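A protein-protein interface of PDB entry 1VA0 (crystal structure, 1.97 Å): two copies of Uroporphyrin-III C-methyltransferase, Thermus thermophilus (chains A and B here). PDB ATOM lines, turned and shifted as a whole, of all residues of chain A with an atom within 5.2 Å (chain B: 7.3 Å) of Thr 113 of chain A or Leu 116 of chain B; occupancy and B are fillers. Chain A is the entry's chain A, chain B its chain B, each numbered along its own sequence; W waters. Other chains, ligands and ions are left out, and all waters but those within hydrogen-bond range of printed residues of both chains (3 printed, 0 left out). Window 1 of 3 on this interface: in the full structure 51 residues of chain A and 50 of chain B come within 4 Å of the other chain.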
ATOM      1  N   PRO A  10       4.414 -13.749  19.511  1.00  0.00           N
ATOM      2  CA  PRO A  10       4.683 -15.186  19.383  1.00  0.00           C
ATOM      3  C   PRO A  10       4.167 -15.901  18.145  1.00  0.00           C
ATOM      4  O   PRO A  10       4.561 -17.034  17.871  1.00  0.00           O
ATOM      5  CB  PRO A  10       4.104 -15.757  20.676  1.00  0.00           C
ATOM      6  CG  PRO A  10       2.926 -14.883  20.923  1.00  0.00           C
ATOM      7  CD  PRO A  10       3.384 -13.479  20.535  1.00  0.00           C
ATOM      8  N   GLY A  84       8.625 -12.662  18.709  1.00  0.00           N
ATOM      9  CA  GLY A  84       8.414 -12.351  20.118  1.00  0.00           C
ATOM     10  C   GLY A  84       8.784 -10.918  20.458  1.00  0.00           C
ATOM     11  O   GLY A  84       8.246  -9.987  19.870  1.00  0.00           O
ATOM     12  N   ASP A  85       9.669 -10.739  21.433  1.00  0.00           N
ATOM     13  CA  ASP A  85      10.136  -9.410  21.804  1.00  0.00           C
ATOM     14  C   ASP A  85      11.527  -9.372  21.182  1.00  0.00           C
ATOM     15  O   ASP A  85      12.287 -10.331  21.299  1.00  0.00           O
ATOM     16  CB  ASP A  85      10.233  -9.260  23.318  1.00  0.00           C
ATOM     17  CG  ASP A  85      10.815  -7.932  23.717  1.00  0.00           C
ATOM     18  OD1 ASP A  85      12.060  -7.808  23.760  1.00  0.00           O
ATOM     19  OD2 ASP A  85      10.028  -6.995  23.970  1.00  0.00           O
ATOM     20  N   VAL A  88      15.148 -10.109  23.623  1.00  0.00           N
ATOM     21  CA  VAL A  88      15.534 -11.318  24.344  1.00  0.00           C
ATOM     22  C   VAL A  88      15.599 -12.478  23.355  1.00  0.00           C
ATOM     23  O   VAL A  88      14.730 -12.619  22.505  1.00  0.00           O
ATOM     24  CB  VAL A  88      14.530 -11.709  25.491  1.00  0.00           C
ATOM     25  CG1 VAL A  88      14.705 -10.788  26.685  1.00  0.00           C
ATOM     26  CG2 VAL A  88      13.085 -11.648  24.983  1.00  0.00           C
ATOM     27  N   PRO A 110       8.944  -3.043  21.998  1.00  0.00           N
ATOM     28  CA  PRO A 110       8.734  -4.313  22.701  1.00  0.00           C
ATOM     29  C   PRO A 110       7.604  -5.129  22.099  1.00  0.00           C
ATOM     30  O   PRO A 110       6.757  -4.604  21.366  1.00  0.00           O
ATOM     31  CB  PRO A 110       8.411  -3.870  24.135  1.00  0.00           C
ATOM     32  CG  PRO A 110       9.158  -2.574  24.263  1.00  0.00           C
ATOM     33  CD  PRO A 110       8.880  -1.906  22.936  1.00  0.00           C
ATOM     34  N   GLY A 111       7.589  -6.419  22.415  1.00  0.00           N
ATOM     35  CA  GLY A 111       6.540  -7.274  21.904  1.00  0.00           C
ATOM     36  C   GLY A 111       6.117  -8.283  22.953  1.00  0.00           C
ATOM     37  O   GLY A 111       6.617  -8.276  24.083  1.00  0.00           O
ATOM     38  N   VAL A 112       5.175  -9.139  22.587  1.00  0.00           N
ATOM     39  CA  VAL A 112       4.711 -10.189  23.478  1.00  0.00           C
ATOM     40  C   VAL A 112       5.753 -11.292  23.282  1.00  0.00           C
ATOM     41  O   VAL A 112       5.838 -11.898  22.216  1.00  0.00           O
ATOM     42  CB  VAL A 112       3.289 -10.682  23.064  1.00  0.00           C
ATOM     43  CG1 VAL A 112       2.917 -11.953  23.843  1.00  0.00           C
ATOM     44  CG2 VAL A 112       2.254  -9.582  23.366  1.00  0.00           C
ATOM     45  N   THR A 113       6.572 -11.531  24.298  1.00  0.00           N
ATOM     46  CA  THR A 113       7.598 -12.549  24.172  1.00  0.00           C
ATOM     47  C   THR A 113       7.024 -13.956  24.101  1.00  0.00           C
ATOM     48  O   THR A 113       5.980 -14.238  24.697  1.00  0.00           O
ATOM     49  CB  THR A 113       8.616 -12.495  25.335  1.00  0.00           C
ATOM     50  OG1 THR A 113       9.500 -13.612  25.228  1.00  0.00           O
ATOM     51  CG2 THR A 113       7.904 -12.514  26.691  1.00  0.00           C
ATOM     52  N   SER A 114       7.712 -14.827  23.358  1.00  0.00           N
ATOM     53  CA  SER A 114       7.304 -16.223  23.191  1.00  0.00           C
ATOM     54  C   SER A 114       7.208 -16.958  24.512  1.00  0.00           C
ATOM     55  O   SER A 114       6.456 -17.923  24.632  1.00  0.00           O
ATOM     56  CB  SER A 114       8.280 -16.939  22.253  1.00  0.00           C
ATOM     57  OG  SER A 114       8.228 -16.306  20.984  1.00  0.00           O
ATOM     58  N   LEU A 115       7.965 -16.484  25.504  1.00  0.00           N
ATOM     59  CA  LEU A 115       7.954 -17.055  26.859  1.00  0.00           C
ATOM     60  C   LEU A 115       6.554 -17.020  27.453  1.00  0.00           C
ATOM     61  O   LEU A 115       6.225 -17.808  28.348  1.00  0.00           O
ATOM     62  CB  LEU A 115       8.808 -16.211  27.799  1.00  0.00           C
ATOM     63  CG  LEU A 115      10.255 -16.091  27.399  1.00  0.00           C
ATOM     64  CD1 LEU A 115      10.921 -14.962  28.166  1.00  0.00           C
ATOM     65  CD2 LEU A 115      10.921 -17.444  27.653  1.00  0.00           C
ATOM     66  N   LEU A 116       5.754 -16.065  26.979  1.00  0.00           N
ATOM     67  CA  LEU A 116       4.406 -15.849  27.493  1.00  0.00           C
ATOM     68  C   LEU A 116       3.330 -16.341  26.547  1.00  0.00           C
ATOM     69  O   LEU A 116       2.165 -16.018  26.731  1.00  0.00           O
ATOM     70  CB  LEU A 116       4.205 -14.343  27.730  1.00  0.00           C
ATOM     71  CG  LEU A 116       5.021 -13.688  28.848  1.00  0.00           C
ATOM     72  CD1 LEU A 116       4.899 -12.164  28.793  1.00  0.00           C
ATOM     73  CD2 LEU A 116       4.526 -14.228  30.176  1.00  0.00           C
ATOM     74  N   ALA A 117       3.721 -17.122  25.542  1.00  0.00           N
ATOM     75  CA  ALA A 117       2.770 -17.586  24.539  1.00  0.00           C
ATOM     76  C   ALA A 117       1.705 -18.581  24.998  1.00  0.00           C
ATOM     77  O   ALA A 117       0.642 -18.639  24.396  1.00  0.00           O
ATOM     78  CB  ALA A 117       3.519 -18.161  23.341  1.00  0.00           C
ATOM     79  N   PRO B  10       3.023  -2.274  29.552  1.00  0.00           N
ATOM     80  CA  PRO B  10       3.702  -1.465  30.569  1.00  0.00           C
ATOM     81  C   PRO B  10       3.169  -0.055  30.816  1.00  0.00           C
ATOM     82  O   PRO B  10       3.501   0.556  31.830  1.00  0.00           O
ATOM     83  CB  PRO B  10       5.144  -1.453  30.076  1.00  0.00           C
ATOM     84  CG  PRO B  10       4.950  -1.377  28.595  1.00  0.00           C
ATOM     85  CD  PRO B  10       3.856  -2.406  28.346  1.00  0.00           C
ATOM     86  N   LEU B  15       1.559   0.124  23.134  1.00  0.00           N
ATOM     87  CA  LEU B  15       2.092  -1.208  23.393  1.00  0.00           C
ATOM     88  C   LEU B  15       1.011  -2.218  23.784  1.00  0.00           C
ATOM     89  O   LEU B  15       1.296  -3.319  24.272  1.00  0.00           O
ATOM     90  CB  LEU B  15       3.219  -1.143  24.440  1.00  0.00           C
ATOM     91  CG  LEU B  15       4.438  -0.347  23.919  1.00  0.00           C
ATOM     92  CD1 LEU B  15       5.585  -0.448  24.884  1.00  0.00           C
ATOM     93  CD2 LEU B  15       4.859  -0.878  22.581  1.00  0.00           C
ATOM     94  N   ASP B  85       1.721  -8.225  31.373  1.00  0.00           N
ATOM     95  CA  ASP B  85       1.138  -9.472  30.890  1.00  0.00           C
ATOM     96  C   ASP B  85       0.406  -9.982  32.133  1.00  0.00           C
ATOM     97  O   ASP B  85       0.968 -10.000  33.215  1.00  0.00           O
ATOM     98  CB  ASP B  85       2.208 -10.480  30.475  1.00  0.00           C
ATOM     99  CG  ASP B  85       1.606 -11.817  30.052  1.00  0.00           C
ATOM    100  OD1 ASP B  85       1.330 -12.669  30.932  1.00  0.00           O
ATOM    101  OD2 ASP B  85       1.389 -12.005  28.836  1.00  0.00           O
ATOM    102  N   PRO B 110      -2.215 -12.407  26.273  1.00  0.00           N
ATOM    103  CA  PRO B 110      -0.860 -12.012  26.686  1.00  0.00           C
ATOM    104  C   PRO B 110      -0.589 -10.549  26.390  1.00  0.00           C
ATOM    105  O   PRO B 110      -1.251  -9.946  25.547  1.00  0.00           O
ATOM    106  CB  PRO B 110       0.038 -12.929  25.860  1.00  0.00           C
ATOM    107  CG  PRO B 110      -0.760 -14.177  25.782  1.00  0.00           C
ATOM    108  CD  PRO B 110      -2.160 -13.639  25.465  1.00  0.00           C
ATOM    109  N   GLY B 111       0.385  -9.980  27.095  1.00  0.00           N
ATOM    110  CA  GLY B 111       0.722  -8.592  26.880  1.00  0.00           C
ATOM    111  C   GLY B 111       2.226  -8.371  26.908  1.00  0.00           C
ATOM    112  O   GLY B 111       3.018  -9.308  27.036  1.00  0.00           O
ATOM    113  N   VAL B 112       2.618  -7.118  26.757  1.00  0.00           N
ATOM    114  CA  VAL B 112       4.021  -6.744  26.814  1.00  0.00           C
ATOM    115  C   VAL B 112       4.309  -6.598  28.301  1.00  0.00           C
ATOM    116  O   VAL B 112       3.837  -5.659  28.927  1.00  0.00           O
ATOM    117  CB  VAL B 112       4.241  -5.395  26.108  1.00  0.00           C
ATOM    118  CG1 VAL B 112       5.672  -4.913  26.316  1.00  0.00           C
ATOM    119  CG2 VAL B 112       3.918  -5.539  24.628  1.00  0.00           C
ATOM    120  N   THR B 113       5.057  -7.529  28.881  1.00  0.00           N
ATOM    121  CA  THR B 113       5.355  -7.448  30.308  1.00  0.00           C
ATOM    122  C   THR B 113       6.290  -6.262  30.586  1.00  0.00           C
ATOM    123  O   THR B 113       7.078  -5.859  29.724  1.00  0.00           O
ATOM    124  CB  THR B 113       5.976  -8.783  30.828  1.00  0.00           C
ATOM    125  OG1 THR B 113       6.278  -8.667  32.226  1.00  0.00           O
ATOM    126  CG2 THR B 113       7.250  -9.133  30.045  1.00  0.00           C
ATOM    127  N   SER B 114       6.177  -5.682  31.776  1.00  0.00           N
ATOM    128  CA  SER B 114       7.018  -4.546  32.143  1.00  0.00           C
ATOM    129  C   SER B 114       8.486  -4.963  32.183  1.00  0.00           C
ATOM    130  O   SER B 114       9.381  -4.136  32.014  1.00  0.00           O
ATOM    131  CB  SER B 114       6.583  -3.975  33.501  1.00  0.00           C
ATOM    132  OG  SER B 114       6.833  -4.904  34.537  1.00  0.00           O
ATOM    133  N   LEU B 115       8.730  -6.258  32.384  1.00  0.00           N
ATOM    134  CA  LEU B 115      10.098  -6.791  32.408  1.00  0.00           C
ATOM    135  C   LEU B 115      10.834  -6.399  31.151  1.00  0.00           C
ATOM    136  O   LEU B 115      12.061  -6.305  31.148  1.00  0.00           O
ATOM    137  CB  LEU B 115      10.102  -8.314  32.434  1.00  0.00           C
ATOM    138  CG  LEU B 115       9.373  -8.965  33.576  1.00  0.00           C
ATOM    139  CD1 LEU B 115       9.355 -10.455  33.354  1.00  0.00           C
ATOM    140  CD2 LEU B 115      10.054  -8.598  34.871  1.00  0.00           C
ATOM    141  N   LEU B 116      10.077  -6.206  30.075  1.00  0.00           N
ATOM    142  CA  LEU B 116      10.646  -5.867  28.774  1.00  0.00           C
ATOM    143  C   LEU B 116      10.469  -4.396  28.406  1.00  0.00           C
ATOM    144  O   LEU B 116      10.703  -4.007  27.263  1.00  0.00           O
ATOM    145  CB  LEU B 116       9.989  -6.743  27.697  1.00  0.00           C
ATOM    146  CG  LEU B 116      10.269  -8.245  27.817  1.00  0.00           C
ATOM    147  CD1 LEU B 116       9.309  -9.072  26.937  1.00  0.00           C
ATOM    148  CD2 LEU B 116      11.715  -8.487  27.418  1.00  0.00           C
ATOM    149  N   ALA B 117      10.067  -3.575  29.371  1.00  0.00           N
ATOM    150  CA  ALA B 117       9.831  -2.166  29.078  1.00  0.00           C
ATOM    151  C   ALA B 117      11.052  -1.268  29.007  1.00  0.00           C
ATOM    152  O   ALA B 117      10.917  -0.118  28.617  1.00  0.00           O
ATOM    153  CB  ALA B 117       8.839  -1.591  30.069  1.00  0.00           C
ATOM    154  N   SER B 118      12.237  -1.759  29.356  1.00  0.00           N
ATOM    155  CA  SER B 118      13.415  -0.882  29.302  1.00  0.00           C
ATOM    156  C   SER B 118      14.052  -0.786  27.913  1.00  0.00           C
ATOM    157  O   SER B 118      14.762   0.172  27.620  1.00  0.00           O
ATOM    158  CB  SER B 118      14.479  -1.330  30.317  1.00  0.00           C
ATOM    159  OG  SER B 118      15.152  -2.500  29.880  1.00  0.00           O
ATOM    160  N   GLY B 119      13.797  -1.771  27.061  1.00  0.00           N
ATOM    161  CA  GLY B 119      14.386  -1.754  25.740  1.00  0.00           C
ATOM    162  C   GLY B 119      15.785  -2.349  25.747  1.00  0.00           C
ATOM    163  O   GLY B 119      16.386  -2.535  24.691  1.00  0.00           O
ATOM    164  N   LEU B 120      16.311  -2.647  26.933  1.00  0.00           N
ATOM    165  CA  LEU B 120      17.646  -3.247  27.040  1.00  0.00           C
ATOM    166  C   LEU B 120      17.607  -4.721  26.648  1.00  0.00           C
ATOM    167  O   LEU B 120      16.580  -5.380  26.804  1.00  0.00           O
ATOM    168  CB  LEU B 120      18.162  -3.133  28.475  1.00  0.00           C
ATOM    169  CG  LEU B 120      18.428  -1.720  29.011  1.00  0.00           C
ATOM    170  CD1 LEU B 120      18.919  -1.819  30.447  1.00  0.00           C
ATOM    171  CD2 LEU B 120      19.470  -1.008  28.141  1.00  0.00           C
ATOM    172  N   LEU B 122      17.950  -8.167  27.537  1.00  0.00           N
ATOM    173  CA  LEU B 122      18.141  -8.934  28.758  1.00  0.00           C
ATOM    174  C   LEU B 122      19.085 -10.109  28.516  1.00  0.00           C
ATOM    175  O   LEU B 122      19.722 -10.606  29.447  1.00  0.00           O
ATOM    176  CB  LEU B 122      16.791  -9.398  29.328  1.00  0.00           C
ATOM    177  CG  LEU B 122      15.801  -8.248  29.604  1.00  0.00           C
ATOM    178  CD1 LEU B 122      14.541  -8.841  30.267  1.00  0.00           C
ATOM    179  CD2 LEU B 122      16.423  -7.178  30.523  1.00  0.00           C
ATOM    180  N   PHE B 131      17.735 -15.061  31.504  1.00  0.00           N
ATOM    181  CA  PHE B 131      17.504 -14.108  32.575  1.00  0.00           C
ATOM    182  C   PHE B 131      16.445 -14.679  33.503  1.00  0.00           C
ATOM    183  O   PHE B 131      15.819 -15.693  33.188  1.00  0.00           O
ATOM    184  CB  PHE B 131      17.053 -12.748  32.001  1.00  0.00           C
ATOM    185  CG  PHE B 131      15.651 -12.748  31.470  1.00  0.00           C
ATOM    186  CD1 PHE B 131      14.572 -12.506  32.318  1.00  0.00           C
ATOM    187  CD2 PHE B 131      15.403 -13.034  30.130  1.00  0.00           C
ATOM    188  CE1 PHE B 131      13.264 -12.552  31.840  1.00  0.00           C
ATOM    189  CE2 PHE B 131      14.089 -13.084  29.633  1.00  0.00           C
ATOM    190  CZ  PHE B 131      13.021 -12.844  30.491  1.00  0.00           C
ATOM    191  N   VAL B 156      15.981  -9.458  36.935  1.00  0.00           N
ATOM    192  CA  VAL B 156      15.017  -8.383  36.963  1.00  0.00           C
ATOM    193  C   VAL B 156      14.158  -8.560  38.215  1.00  0.00           C
ATOM    194  O   VAL B 156      13.658  -9.653  38.498  1.00  0.00           O
ATOM    195  CB  VAL B 156      14.141  -8.418  35.694  1.00  0.00           C
ATOM    196  CG1 VAL B 156      13.243  -7.189  35.651  1.00  0.00           C
ATOM    197  CG2 VAL B 156      15.046  -8.463  34.457  1.00  0.00           C
ATOM    198  N   ALA B 188       8.213   3.093  33.834  1.00  0.00           N
ATOM    199  CA  ALA B 188       8.691   2.812  32.501  1.00  0.00           C
ATOM    200  C   ALA B 188       7.505   2.885  31.526  1.00  0.00           C
ATOM    201  O   ALA B 188       6.378   2.594  31.866  1.00  0.00           O
ATOM    202  CB  ALA B 188       9.314   1.432  32.449  1.00  0.00           C
ATOM    203  N   LEU B 215      10.954  -0.782  37.764  1.00  0.00           N
ATOM    204  CA  LEU B 215      11.513  -2.035  37.266  1.00  0.00           C
ATOM    205  C   LEU B 215      12.983  -1.959  37.695  1.00  0.00           C
ATOM    206  O   LEU B 215      13.588  -0.888  37.618  1.00  0.00           O
ATOM    207  CB  LEU B 215      11.400  -2.052  35.737  1.00  0.00           C
ATOM    208  CG  LEU B 215      12.150  -3.072  34.877  1.00  0.00           C
ATOM    209  CD1 LEU B 215      11.574  -4.459  35.086  1.00  0.00           C
ATOM    210  CD2 LEU B 215      12.012  -2.672  33.417  1.00  0.00           C
ATOM    211  N   ILE B 217      16.667  -3.693  37.020  1.00  0.00           N
ATOM    212  CA  ILE B 217      17.466  -4.637  36.253  1.00  0.00           C
ATOM    213  C   ILE B 217      18.910  -4.668  36.752  1.00  0.00           C
ATOM    214  O   ILE B 217      19.541  -3.620  36.936  1.00  0.00           O
ATOM    215  CB  ILE B 217      17.439  -4.277  34.766  1.00  0.00           C
ATOM    216  CG1 ILE B 217      15.977  -4.234  34.290  1.00  0.00           C
ATOM    217  CG2 ILE B 217      18.240  -5.314  33.962  1.00  0.00           C
ATOM    218  CD1 ILE B 217      15.758  -3.591  32.943  1.00  0.00           C
HETATM  219  O   HOH W   1      12.262  -5.113  25.168  1.00  0.00           O
HETATM  220  O   HOH W   2       5.906  -9.668  26.718  1.00  0.00           O
HETATM  221  O   HOH W   3       0.810 -14.930  29.232  1.00  0.00           O
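Asp 85 of chain A touches Leu 116 of chain B, and with the chains exchanged Leu 116 of chain A touches Asp 85 of chain B. Pro 110 of chain A touches Val 112 of chain B, and with the chains exchanged Val 112 of chain A touches Pro 110 of chain B. Pro 110 of chain A touches Leu 116 of chain B, and with the chains exchanged Leu 116 of chain A touches Pro 110 of chain B. Gly 111 of chain A touches Val 112 of chain B, and with the chains exchanged Val 112 of chain A touches Gly 111 of chain B. 10 positions are printed for both chains. Of the 14 pairs that touch across the chains among the printed residues, 8 have their exchanged pair printed and touching as well.
Among the printed residues, pairs that only touch across the chains: Asp 85 of chain A with Leu 116 of chain B (3.7 Å), Val 88 of chain A with Leu 116 of chain B (3.8 Å), Val 88 of chain A with Leu 122 of chain B (3.6 Å), Val 88 of chain A with Phe 131 of chain B (3.8 Å), Pro 110 of chain A with Val 112 of chain B (3.7 Å), Pro 110 of chain A with Leu 116 of chain B (3.7 Å), Gly 111 of chain A with Val 112 of chain B (3.9 Å), Val 112 of chain A with Pro 110 of chain B (3.6 Å), Val 112 of chain A with Gly 111 of chain B (3.7 Å), Thr 113 of chain A with Leu 116 of chain B (3.7 Å), Leu 115 of chain A with Phe 131 of chain B (3.8 Å), Leu 116 of chain A with Asp 85 of chain B (3.5 Å), Leu 116 of chain A with Pro 110 of chain B (3.6 Å) and Leu 116 of chain A with Gly 111 of chain B (3.8 Å).
Water W1 bridges the backbone carbonyl oxygen (O) of Leu 116 of chain B and the side-chain carboxylate (OD1) of Asp 85 of chain A. Water W3 bridges OD1 of Asp 85 of chain B (2.9 Å) and O of Leu 116 of chain A (3.0 Å). Water W2 lies within hydrogen-bond range of O of Gly 111 of chain B (2.9 Å), O of Gly 111 of chain A (3.1 Å), N of Thr 113 of chain A (3.1 Å) and N of Thr 113 of chain B (3.2 Å).
Hydrophobic or aromatic side chains of chain A that line the printed part of chain B: Val 88, Pro 110, Val 112, Leu 115 and Leu 116. Along chain A the printed residues that touch a printed residue of chain B span positions 85 to 116. Among the printed residues, no Asp or Glu carboxylate lies within 4 Å of a Lys or Arg side-chain nitrogen of the other chain.
Of the printed residues of chain B, Asp 85 of chain A touches Leu 116 (3.7 Å). Thr 113 of chain A touches just one residue of chain B: Leu 116 (3.7 Å). Printed residues of chain A within 4 Å of Asp 85 of chain B: Leu 116. Of the printed residues of chain A, Pro 110 of chain B touches Val 112 and Leu 116. Printed residues of chain A within 4 Å of Gly 111 of chain B: Val 112 (3.7 Å) and Leu 116 (3.8 Å). Thr 113 of chain B touches none of the printed residues of chain A. Printed residues of chain A within 4 Å of Leu 122 of chain B: Val 88. The nearest residue of chain B that does not touch Thr 113 of chain A is Thr 113 of chain B (4.8 Å). The nearest printed residue of chain A that does not touch Gly 111 of chain B is Gly 111 of chain A (4.8 Å).
The backbone NH of Gly 111 of chain A sits at hydrogen-bond distance from the side-chain carboxylate of Asp 85 of chain A, 2.9 Å away. OG1 of Thr 113 of chain A lies close to N of Leu 115 of chain A. The backbone NH (N) of Gly 111 of chain B lies within hydrogen-bond range of the side-chain carboxylate (OD2) of Asp 85 of chain B.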
